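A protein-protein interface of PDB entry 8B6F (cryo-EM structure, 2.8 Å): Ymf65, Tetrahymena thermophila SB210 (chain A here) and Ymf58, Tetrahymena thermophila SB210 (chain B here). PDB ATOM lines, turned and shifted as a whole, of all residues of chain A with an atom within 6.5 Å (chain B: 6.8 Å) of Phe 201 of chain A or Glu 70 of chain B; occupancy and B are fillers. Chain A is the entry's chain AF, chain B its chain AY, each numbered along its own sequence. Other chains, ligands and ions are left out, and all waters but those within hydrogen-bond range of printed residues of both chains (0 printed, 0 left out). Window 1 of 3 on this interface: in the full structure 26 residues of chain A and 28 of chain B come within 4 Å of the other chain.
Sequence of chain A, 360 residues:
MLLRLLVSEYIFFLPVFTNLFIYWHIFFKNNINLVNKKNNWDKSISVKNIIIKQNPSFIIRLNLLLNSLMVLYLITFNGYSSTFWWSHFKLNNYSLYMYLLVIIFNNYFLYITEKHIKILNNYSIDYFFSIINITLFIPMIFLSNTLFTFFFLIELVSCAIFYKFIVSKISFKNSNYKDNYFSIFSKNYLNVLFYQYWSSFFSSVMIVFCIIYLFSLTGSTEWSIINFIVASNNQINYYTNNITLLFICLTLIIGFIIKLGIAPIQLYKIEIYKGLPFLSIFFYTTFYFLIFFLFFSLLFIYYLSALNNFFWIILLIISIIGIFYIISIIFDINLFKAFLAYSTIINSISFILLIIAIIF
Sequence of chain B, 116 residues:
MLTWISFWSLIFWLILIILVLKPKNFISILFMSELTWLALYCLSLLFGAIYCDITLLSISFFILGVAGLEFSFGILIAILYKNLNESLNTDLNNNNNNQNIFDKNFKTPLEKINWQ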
ATOM      1  N   GLU A 155      21.926  17.650  25.382  1.00  0.00           N
ATOM      2  CA  GLU A 155      23.242  18.272  25.447  1.00  0.00           C
ATOM      3  C   GLU A 155      24.325  17.238  25.726  1.00  0.00           C
ATOM      4  O   GLU A 155      25.400  17.275  25.118  1.00  0.00           O
ATOM      5  CB  GLU A 155      23.252  19.358  26.523  1.00  0.00           C
ATOM      6  CG  GLU A 155      24.466  20.268  26.481  1.00  0.00           C
ATOM      7  CD  GLU A 155      24.455  21.203  25.286  1.00  0.00           C
ATOM      8  OE1 GLU A 155      23.463  21.194  24.530  1.00  0.00           O
ATOM      9  OE2 GLU A 155      25.441  21.948  25.102  1.00  0.00           O
ATOM     10  N   GLN A 196      29.392  21.116  13.253  1.00  0.00           N
ATOM     11  CA  GLN A 196      28.741  20.451  14.376  1.00  0.00           C
ATOM     12  C   GLN A 196      28.722  21.358  15.598  1.00  0.00           C
ATOM     13  O   GLN A 196      27.701  21.480  16.283  1.00  0.00           O
ATOM     14  CB  GLN A 196      29.451  19.131  14.688  1.00  0.00           C
ATOM     15  CG  GLN A 196      28.853  18.346  15.852  1.00  0.00           C
ATOM     16  CD  GLN A 196      27.434  17.882  15.589  1.00  0.00           C
ATOM     17  OE1 GLN A 196      26.911  18.031  14.487  1.00  0.00           O
ATOM     18  NE2 GLN A 196      26.803  17.312  16.609  1.00  0.00           N
ATOM     19  N   TYR A 197      29.855  21.996  15.892  1.00  0.00           N
ATOM     20  CA  TYR A 197      29.945  22.846  17.074  1.00  0.00           C
ATOM     21  C   TYR A 197      28.974  24.019  16.995  1.00  0.00           C
ATOM     22  O   TYR A 197      28.278  24.328  17.969  1.00  0.00           O
ATOM     23  CB  TYR A 197      31.382  23.343  17.236  1.00  0.00           C
ATOM     24  CG  TYR A 197      31.566  24.393  18.307  1.00  0.00           C
ATOM     25  CD1 TYR A 197      31.768  24.040  19.633  1.00  0.00           C
ATOM     26  CD2 TYR A 197      31.564  25.742  17.982  1.00  0.00           C
ATOM     27  CE1 TYR A 197      31.945  25.002  20.608  1.00  0.00           C
ATOM     28  CE2 TYR A 197      31.741  26.710  18.946  1.00  0.00           C
ATOM     29  CZ  TYR A 197      31.932  26.336  20.257  1.00  0.00           C
ATOM     30  OH  TYR A 197      32.107  27.303  21.219  1.00  0.00           O
ATOM     31  N   TRP A 198      28.912  24.685  15.842  1.00  0.00           N
ATOM     32  CA  TRP A 198      28.086  25.884  15.746  1.00  0.00           C
ATOM     33  C   TRP A 198      26.605  25.550  15.652  1.00  0.00           C
ATOM     34  O   TRP A 198      25.767  26.285  16.186  1.00  0.00           O
ATOM     35  CB  TRP A 198      28.533  26.736  14.561  1.00  0.00           C
ATOM     36  CG  TRP A 198      29.847  27.372  14.834  1.00  0.00           C
ATOM     37  CD1 TRP A 198      31.012  27.173  14.162  1.00  0.00           C
ATOM     38  CD2 TRP A 198      30.144  28.284  15.896  1.00  0.00           C
ATOM     39  NE1 TRP A 198      32.017  27.917  14.730  1.00  0.00           N
ATOM     40  CE2 TRP A 198      31.508  28.609  15.796  1.00  0.00           C
ATOM     41  CE3 TRP A 198      29.385  28.862  16.919  1.00  0.00           C
ATOM     42  CZ2 TRP A 198      32.130  29.489  16.677  1.00  0.00           C
ATOM     43  CZ3 TRP A 198      30.001  29.736  17.788  1.00  0.00           C
ATOM     44  CH2 TRP A 198      31.362  30.040  17.665  1.00  0.00           C
ATOM     45  N   SER A 199      26.259  24.453  14.982  1.00  0.00           N
ATOM     46  CA  SER A 199      24.876  23.997  15.000  1.00  0.00           C
ATOM     47  C   SER A 199      24.436  23.666  16.415  1.00  0.00           C
ATOM     48  O   SER A 199      23.322  24.004  16.826  1.00  0.00           O
ATOM     49  CB  SER A 199      24.719  22.794  14.079  1.00  0.00           C
ATOM     50  OG  SER A 199      25.117  23.154  12.773  1.00  0.00           O
ATOM     51  N   SER A 200      25.297  22.990  17.175  1.00  0.00           N
ATOM     52  CA  SER A 200      24.968  22.699  18.564  1.00  0.00           C
ATOM     53  C   SER A 200      24.779  23.986  19.351  1.00  0.00           C
ATOM     54  O   SER A 200      23.851  24.097  20.161  1.00  0.00           O
ATOM     55  CB  SER A 200      26.063  21.838  19.194  1.00  0.00           C
ATOM     56  OG  SER A 200      26.181  20.595  18.522  1.00  0.00           O
ATOM     57  N   PHE A 201      25.653  24.971  19.134  1.00  0.00           N
ATOM     58  CA  PHE A 201      25.526  26.235  19.847  1.00  0.00           C
ATOM     59  C   PHE A 201      24.187  26.901  19.556  1.00  0.00           C
ATOM     60  O   PHE A 201      23.468  27.302  20.477  1.00  0.00           O
ATOM     61  CB  PHE A 201      26.675  27.171  19.474  1.00  0.00           C
ATOM     62  CG  PHE A 201      26.377  28.614  19.740  1.00  0.00           C
ATOM     63  CD1 PHE A 201      26.501  29.131  21.017  1.00  0.00           C
ATOM     64  CD2 PHE A 201      25.967  29.453  18.719  1.00  0.00           C
ATOM     65  CE1 PHE A 201      26.223  30.458  21.272  1.00  0.00           C
ATOM     66  CE2 PHE A 201      25.687  30.781  18.967  1.00  0.00           C
ATOM     67  CZ  PHE A 201      25.815  31.284  20.246  1.00  0.00           C
ATOM     68  N   PHE A 202      23.833  27.029  18.274  1.00  0.00           N
ATOM     69  CA  PHE A 202      22.580  27.691  17.919  1.00  0.00           C
ATOM     70  C   PHE A 202      21.386  26.952  18.500  1.00  0.00           C
ATOM     71  O   PHE A 202      20.487  27.560  19.089  1.00  0.00           O
ATOM     72  CB  PHE A 202      22.454  27.800  16.401  1.00  0.00           C
ATOM     73  CG  PHE A 202      23.236  28.931  15.810  1.00  0.00           C
ATOM     74  CD1 PHE A 202      22.850  30.240  16.031  1.00  0.00           C
ATOM     75  CD2 PHE A 202      24.345  28.686  15.021  1.00  0.00           C
ATOM     76  CE1 PHE A 202      23.563  31.287  15.484  1.00  0.00           C
ATOM     77  CE2 PHE A 202      25.062  29.728  14.471  1.00  0.00           C
ATOM     78  CZ  PHE A 202      24.671  31.030  14.704  1.00  0.00           C
ATOM     79  N   SER A 203      21.350  25.633  18.330  1.00  0.00           N
ATOM     80  CA  SER A 203      20.230  24.859  18.846  1.00  0.00           C
ATOM     81  C   SER A 203      20.127  24.991  20.358  1.00  0.00           C
ATOM     82  O   SER A 203      19.029  25.136  20.905  1.00  0.00           O
ATOM     83  CB  SER A 203      20.389  23.396  18.443  1.00  0.00           C
ATOM     84  OG  SER A 203      21.609  22.883  18.946  1.00  0.00           O
ATOM     85  N   SER A 204      21.264  24.935  21.054  1.00  0.00           N
ATOM     86  CA  SER A 204      21.245  25.001  22.511  1.00  0.00           C
ATOM     87  C   SER A 204      20.751  26.354  23.006  1.00  0.00           C
ATOM     88  O   SER A 204      19.916  26.423  23.914  1.00  0.00           O
ATOM     89  CB  SER A 204      22.639  24.706  23.064  1.00  0.00           C
ATOM     90  OG  SER A 204      23.075  23.413  22.681  1.00  0.00           O
ATOM     91  N   VAL A 205      21.248  27.446  22.423  1.00  0.00           N
ATOM     92  CA  VAL A 205      20.820  28.764  22.883  1.00  0.00           C
ATOM     93  C   VAL A 205      19.332  28.959  22.627  1.00  0.00           C
ATOM     94  O   VAL A 205      18.604  29.475  23.483  1.00  0.00           O
ATOM     95  CB  VAL A 205      21.663  29.874  22.224  1.00  0.00           C
ATOM     96  CG1 VAL A 205      23.115  29.752  22.644  1.00  0.00           C
ATOM     97  CG2 VAL A 205      21.535  29.842  20.708  1.00  0.00           C
ATOM     98  N   MET A 206      18.856  28.559  21.447  1.00  0.00           N
ATOM     99  CA  MET A 206      17.441  28.734  21.141  1.00  0.00           C
ATOM    100  C   MET A 206      16.568  27.873  22.046  1.00  0.00           C
ATOM    101  O   MET A 206      15.500  28.312  22.484  1.00  0.00           O
ATOM    102  CB  MET A 206      17.183  28.419  19.669  1.00  0.00           C
ATOM    103  CG  MET A 206      17.897  29.379  18.730  1.00  0.00           C
ATOM    104  SD  MET A 206      17.423  29.207  17.005  1.00  0.00           S
ATOM    105  CE  MET A 206      15.734  29.795  17.087  1.00  0.00           C
ATOM    106  N   LEU B  16      22.722  37.897  18.898  1.00  0.00           N
ATOM    107  CA  LEU B  16      22.797  36.899  17.838  1.00  0.00           C
ATOM    108  C   LEU B  16      23.009  37.562  16.484  1.00  0.00           C
ATOM    109  O   LEU B  16      23.774  37.063  15.651  1.00  0.00           O
ATOM    110  CB  LEU B  16      21.529  36.044  17.832  1.00  0.00           C
ATOM    111  CG  LEU B  16      21.462  34.949  18.900  1.00  0.00           C
ATOM    112  CD1 LEU B  16      20.087  34.315  18.922  1.00  0.00           C
ATOM    113  CD2 LEU B  16      22.527  33.891  18.671  1.00  0.00           C
ATOM    114  N   LEU B  19      26.599  38.524  16.227  1.00  0.00           N
ATOM    115  CA  LEU B  19      27.418  37.347  15.964  1.00  0.00           C
ATOM    116  C   LEU B  19      27.406  37.000  14.482  1.00  0.00           C
ATOM    117  O   LEU B  19      28.456  36.745  13.882  1.00  0.00           O
ATOM    118  CB  LEU B  19      26.917  36.171  16.807  1.00  0.00           C
ATOM    119  CG  LEU B  19      27.602  34.808  16.660  1.00  0.00           C
ATOM    120  CD1 LEU B  19      27.382  33.991  17.915  1.00  0.00           C
ATOM    121  CD2 LEU B  19      27.089  34.024  15.460  1.00  0.00           C
ATOM    122  N   ILE B  29      33.784  34.883  16.714  1.00  0.00           N
ATOM    123  CA  ILE B  29      32.521  34.165  16.852  1.00  0.00           C
ATOM    124  C   ILE B  29      32.456  33.481  18.211  1.00  0.00           C
ATOM    125  O   ILE B  29      31.390  33.400  18.832  1.00  0.00           O
ATOM    126  CB  ILE B  29      32.335  33.152  15.707  1.00  0.00           C
ATOM    127  CG1 ILE B  29      32.589  33.816  14.351  1.00  0.00           C
ATOM    128  CG2 ILE B  29      30.906  32.638  15.723  1.00  0.00           C
ATOM    129  CD1 ILE B  29      32.424  32.889  13.156  1.00  0.00           C
ATOM    130  N   LEU B  30      33.593  32.975  18.693  1.00  0.00           N
ATOM    131  CA  LEU B  30      33.629  32.363  20.016  1.00  0.00           C
ATOM    132  C   LEU B  30      33.311  33.384  21.102  1.00  0.00           C
ATOM    133  O   LEU B  30      32.558  33.088  22.037  1.00  0.00           O
ATOM    134  CB  LEU B  30      34.999  31.730  20.255  1.00  0.00           C
ATOM    135  CG  LEU B  30      35.154  30.825  21.479  1.00  0.00           C
ATOM    136  CD1 LEU B  30      34.266  29.597  21.368  1.00  0.00           C
ATOM    137  CD2 LEU B  30      36.607  30.423  21.655  1.00  0.00           C
ATOM    138  N   MET B  32      31.522  36.092  20.729  1.00  0.00           N
ATOM    139  CA  MET B  32      30.107  36.424  20.601  1.00  0.00           C
ATOM    140  C   MET B  32      29.224  35.318  21.166  1.00  0.00           C
ATOM    141  O   MET B  32      28.182  35.597  21.768  1.00  0.00           O
ATOM    142  CB  MET B  32      29.759  36.688  19.136  1.00  0.00           C
ATOM    143  CG  MET B  32      30.456  37.902  18.537  1.00  0.00           C
ATOM    144  SD  MET B  32      30.119  39.437  19.422  1.00  0.00           S
ATOM    145  CE  MET B  32      28.344  39.551  19.241  1.00  0.00           C
ATOM    146  N   SER B  33      29.619  34.058  20.979  1.00  0.00           N
ATOM    147  CA  SER B  33      28.863  32.960  21.572  1.00  0.00           C
ATOM    148  C   SER B  33      28.898  33.036  23.092  1.00  0.00           C
ATOM    149  O   SER B  33      27.882  32.796  23.755  1.00  0.00           O
ATOM    150  CB  SER B  33      29.416  31.619  21.091  1.00  0.00           C
ATOM    151  OG  SER B  33      30.755  31.441  21.511  1.00  0.00           O
ATOM    152  N   GLU B  34      30.057  33.363  23.664  1.00  0.00           N
ATOM    153  CA  GLU B  34      30.134  33.543  25.110  1.00  0.00           C
ATOM    154  C   GLU B  34      29.213  34.665  25.567  1.00  0.00           C
ATOM    155  O   GLU B  34      28.525  34.537  26.586  1.00  0.00           O
ATOM    156  CB  GLU B  34      31.577  33.830  25.524  1.00  0.00           C
ATOM    157  CG  GLU B  34      31.781  33.948  27.026  1.00  0.00           C
ATOM    158  CD  GLU B  34      31.423  32.674  27.764  1.00  0.00           C
ATOM    159  OE1 GLU B  34      31.364  31.607  27.119  1.00  0.00           O
ATOM    160  OE2 GLU B  34      31.196  32.741  28.990  1.00  0.00           O
ATOM    161  N   THR B  36      26.492  35.649  24.097  1.00  0.00           N
ATOM    162  CA  THR B  36      25.122  35.157  23.985  1.00  0.00           C
ATOM    163  C   THR B  36      24.746  34.295  25.182  1.00  0.00           C
ATOM    164  O   THR B  36      23.643  34.423  25.725  1.00  0.00           O
ATOM    165  CB  THR B  36      24.951  34.363  22.690  1.00  0.00           C
ATOM    166  OG1 THR B  36      25.360  35.163  21.573  1.00  0.00           O
ATOM    167  CG2 THR B  36      23.498  33.947  22.503  1.00  0.00           C
ATOM    168  N   TRP B  37      25.647  33.412  25.611  1.00  0.00           N
ATOM    169  CA  TRP B  37      25.371  32.598  26.789  1.00  0.00           C
ATOM    170  C   TRP B  37      25.155  33.471  28.016  1.00  0.00           C
ATOM    171  O   TRP B  37      24.266  33.200  28.830  1.00  0.00           O
ATOM    172  CB  TRP B  37      26.513  31.612  27.030  1.00  0.00           C
ATOM    173  CG  TRP B  37      26.421  30.378  26.197  1.00  0.00           C
ATOM    174  CD1 TRP B  37      27.299  29.971  25.238  1.00  0.00           C
ATOM    175  CD2 TRP B  37      25.389  29.386  26.245  1.00  0.00           C
ATOM    176  NE1 TRP B  37      26.878  28.785  24.687  1.00  0.00           N
ATOM    177  CE2 TRP B  37      25.709  28.405  25.289  1.00  0.00           C
ATOM    178  CE3 TRP B  37      24.226  29.234  27.007  1.00  0.00           C
ATOM    179  CZ2 TRP B  37      24.907  27.286  25.072  1.00  0.00           C
ATOM    180  CZ3 TRP B  37      23.432  28.124  26.793  1.00  0.00           C
ATOM    181  CH2 TRP B  37      23.775  27.163  25.832  1.00  0.00           C
ATOM    182  N   GLY B  65      28.310  26.458  33.094  1.00  0.00           N
ATOM    183  CA  GLY B  65      29.051  25.249  32.773  1.00  0.00           C
ATOM    184  C   GLY B  65      29.010  24.900  31.301  1.00  0.00           C
ATOM    185  O   GLY B  65      30.028  24.522  30.716  1.00  0.00           O
ATOM    186  N   VAL B  66      27.836  25.008  30.682  1.00  0.00           N
ATOM    187  CA  VAL B  66      27.736  24.721  29.255  1.00  0.00           C
ATOM    188  C   VAL B  66      28.586  25.708  28.467  1.00  0.00           C
ATOM    189  O   VAL B  66      29.270  25.335  27.506  1.00  0.00           O
ATOM    190  CB  VAL B  66      26.264  24.739  28.806  1.00  0.00           C
ATOM    191  CG1 VAL B  66      26.155  24.588  27.296  1.00  0.00           C
ATOM    192  CG2 VAL B  66      25.492  23.636  29.508  1.00  0.00           C
ATOM    193  N   ALA B  67      28.552  26.984  28.857  1.00  0.00           N
ATOM    194  CA  ALA B  67      29.374  27.980  28.180  1.00  0.00           C
ATOM    195  C   ALA B  67      30.857  27.675  28.344  1.00  0.00           C
ATOM    196  O   ALA B  67      31.635  27.819  27.395  1.00  0.00           O
ATOM    197  CB  ALA B  67      29.056  29.375  28.718  1.00  0.00           C
ATOM    198  N   GLY B  68      31.267  27.254  29.540  1.00  0.00           N
ATOM    199  CA  GLY B  68      32.663  26.903  29.743  1.00  0.00           C
ATOM    200  C   GLY B  68      33.103  25.737  28.881  1.00  0.00           C
ATOM    201  O   GLY B  68      34.179  25.769  28.281  1.00  0.00           O
ATOM    202  N   LEU B  69      32.278  24.691  28.807  1.00  0.00           N
ATOM    203  CA  LEU B  69      32.622  23.545  27.973  1.00  0.00           C
ATOM    204  C   LEU B  69      32.707  23.940  26.505  1.00  0.00           C
ATOM    205  O   LEU B  69      33.630  23.527  25.795  1.00  0.00           O
ATOM    206  CB  LEU B  69      31.602  22.426  28.172  1.00  0.00           C
ATOM    207  CG  LEU B  69      31.843  21.152  27.359  1.00  0.00           C
ATOM    208  CD1 LEU B  69      33.191  20.528  27.690  1.00  0.00           C
ATOM    209  CD2 LEU B  69      30.722  20.158  27.598  1.00  0.00           C
ATOM    210  N   GLU B  70      31.747  24.737  26.030  1.00  0.00           N
ATOM    211  CA  GLU B  70      31.774  25.173  24.638  1.00  0.00           C
ATOM    212  C   GLU B  70      32.987  26.051  24.365  1.00  0.00           C
ATOM    213  O   GLU B  70      33.582  25.984  23.284  1.00  0.00           O
ATOM    214  CB  GLU B  70      30.483  25.909  24.287  1.00  0.00           C
ATOM    215  CG  GLU B  70      29.272  24.997  24.200  1.00  0.00           C
ATOM    216  CD  GLU B  70      28.070  25.680  23.578  1.00  0.00           C
ATOM    217  OE1 GLU B  70      28.191  26.860  23.186  1.00  0.00           O
ATOM    218  OE2 GLU B  70      27.003  25.037  23.479  1.00  0.00           O
ATOM    219  N   PHE B  71      33.372  26.881  25.336  1.00  0.00           N
ATOM    220  CA  PHE B  71      34.552  27.718  25.164  1.00  0.00           C
ATOM    221  C   PHE B  71      35.814  26.869  25.092  1.00  0.00           C
ATOM    222  O   PHE B  71      36.723  27.165  24.308  1.00  0.00           O
ATOM    223  CB  PHE B  71      34.648  28.735  26.302  1.00  0.00           C
ATOM    224  CG  PHE B  71      35.441  29.962  25.949  1.00  0.00           C
ATOM    225  CD1 PHE B  71      34.836  31.027  25.303  1.00  0.00           C
ATOM    226  CD2 PHE B  71      36.786  30.052  26.267  1.00  0.00           C
ATOM    227  CE1 PHE B  71      35.558  32.160  24.976  1.00  0.00           C
ATOM    228  CE2 PHE B  71      37.514  31.182  25.943  1.00  0.00           C
ATOM    229  CZ  PHE B  71      36.899  32.237  25.298  1.00  0.00           C
ATOM    230  N   SER B  72      35.889  25.810  25.897  1.00  0.00           N
ATOM    231  CA  SER B  72      37.023  24.898  25.808  1.00  0.00           C
ATOM    232  C   SER B  72      37.100  24.261  24.428  1.00  0.00           C
ATOM    233  O   SER B  72      38.175  24.181  23.826  1.00  0.00           O
ATOM    234  CB  SER B  72      36.906  23.820  26.886  1.00  0.00           C
ATOM    235  OG  SER B  72      36.934  24.387  28.183  1.00  0.00           O
ATOM    236  N   PHE B  73      35.963  23.787  23.914  1.00  0.00           N
ATOM    237  CA  PHE B  73      35.944  23.205  22.577  1.00  0.00           C
ATOM    238  C   PHE B  73      36.352  24.230  21.530  1.00  0.00           C
ATOM    239  O   PHE B  73      37.081  23.908  20.584  1.00  0.00           O
ATOM    240  CB  PHE B  73      34.557  22.642  22.266  1.00  0.00           C
ATOM    241  CG  PHE B  73      34.263  21.335  22.946  1.00  0.00           C
ATOM    242  CD1 PHE B  73      35.197  20.312  22.951  1.00  0.00           C
ATOM    243  CD2 PHE B  73      33.051  21.130  23.580  1.00  0.00           C
ATOM    244  CE1 PHE B  73      34.928  19.111  23.572  1.00  0.00           C
ATOM    245  CE2 PHE B  73      32.775  19.929  24.205  1.00  0.00           C
ATOM    246  CZ  PHE B  73      33.715  18.919  24.201  1.00  0.00           C
ATOM    247  N   GLY B  74      35.895  25.472  21.684  1.00  0.00           N
ATOM    248  CA  GLY B  74      36.267  26.510  20.738  1.00  0.00           C
ATOM    249  C   GLY B  74      37.752  26.808  20.749  1.00  0.00           C
ATOM    250  O   GLY B  74      38.363  27.002  19.695  1.00  0.00           O
ATOM    251  N   ILE B  75      38.357  26.849  21.935  1.00  0.00           N
ATOM    252  CA  ILE B  75      39.801  27.044  22.017  1.00  0.00           C
ATOM    253  C   ILE B  75      40.523  25.923  21.284  1.00  0.00           C
ATOM    254  O   ILE B  75      41.469  26.160  20.524  1.00  0.00           O
ATOM    255  CB  ILE B  75      40.245  27.128  23.488  1.00  0.00           C
ATOM    256  CG1 ILE B  75      39.738  28.426  24.119  1.00  0.00           C
ATOM    257  CG2 ILE B  75      41.767  27.030  23.604  1.00  0.00           C
ATOM    258  CD1 ILE B  75      39.955  28.508  25.613  1.00  0.00           C
ATOM    259  N   ILE B  77      39.439  23.989  18.845  1.00  0.00           N
ATOM    260  CA  ILE B  77      39.255  24.084  17.400  1.00  0.00           C
ATOM    261  C   ILE B  77      40.098  25.216  16.830  1.00  0.00           C
ATOM    262  O   ILE B  77      40.705  25.077  15.762  1.00  0.00           O
ATOM    263  CB  ILE B  77      37.764  24.255  17.056  1.00  0.00           C
ATOM    264  CG1 ILE B  77      36.967  23.033  17.518  1.00  0.00           C
ATOM    265  CG2 ILE B  77      37.579  24.456  15.554  1.00  0.00           C
ATOM    266  CD1 ILE B  77      35.465  23.221  17.464  1.00  0.00           C
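Of the 21 printed residues of chain B, 8 touch a printed residue of chain A. Of the 12 printed residues of chain A, 7 touch a printed residue of chain B. Hydrophobic or aromatic side chains of chain A within 4 Å of the printed part of chain B: Tyr 197, Trp 198, Phe 201, Phe 202 and Val 205. Among the printed residues, 15 pairs touch across the chains. Among the printed residues, no Asp or Glu carboxylate lies within 4 Å of a Lys or Arg side-chain nitrogen of the other chain.
OH of Tyr 197 of chain A sits at hydrogen-bond distance from O of Glu 70 of chain B, 2.9 Å away.
The side-chain carboxylate (OE1) of Glu 155 of chain A is in hydrogen-bond range of the side-chain hydroxyl (OG) of Ser 204 of chain A (2.9 Å). The backbone carbonyl oxygen of Ser 200 of chain A lies within hydrogen-bond range of the side-chain hydroxyl of Ser 204 of chain A. The backbone carbonyl oxygen (O) of Ile 29 of chain B sits at hydrogen-bond distance from the side-chain hydroxyl (OG) of Ser 33 of chain B (3.4 Å). O of Leu 30 of chain B lies within hydrogen-bond range of OG of Ser 33 of chain B (2.5 Å). OE1 of Glu 70 of chain B is in hydrogen-bond range of NE1 of Trp 37 of chain B, at 2.8 Å.
Among the printed residues, pairs that only touch across the chains: Tyr 197 of chain A with Leu 30 of chain B, Trp 198 of chain A with Ile 29 of chain B, Phe 201 of chain A with Ser 33 of chain B, Glu 155 of chain A with Val 66 of chain B, Phe 201 of chain A with Glu 70 of chain B, Phe 201 of chain A with Trp 37 of chain B, Phe 201 of chain A with Leu 19 of chain B, Glu 155 of chain A with Glu 70 of chain B, Trp 198 of chain A with Leu 30 of chain B, Trp 198 of chain A with Ser 33 of chain B, Ser 204 of chain A with Trp 37 of chain B, Tyr 197 of chain A with Phe 73 of chain B, Val 205 of chain A with Trp 37 of chain B and Phe 202 of chain A with Leu 19 of chain B.
Phe 201 of chain A touches four residues of chain B. Glu 70 of chain B touches three residues of chain A. Printed residues of chain B within 4 Å of Tyr 197 of chain A: Leu 30, Glu 70 and Phe 73. Printed residues of chain B within 4 Å of Val 205 of chain A: Trp 37 (3.9 Å). Printed residues of chain B within 4 Å of Trp 198 of chain A: Ile 29, Leu 30 and Ser 33. The nearest residue of chain B that does not touch Phe 201 of chain A is Thr 36 of chain B (4.02 Å).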
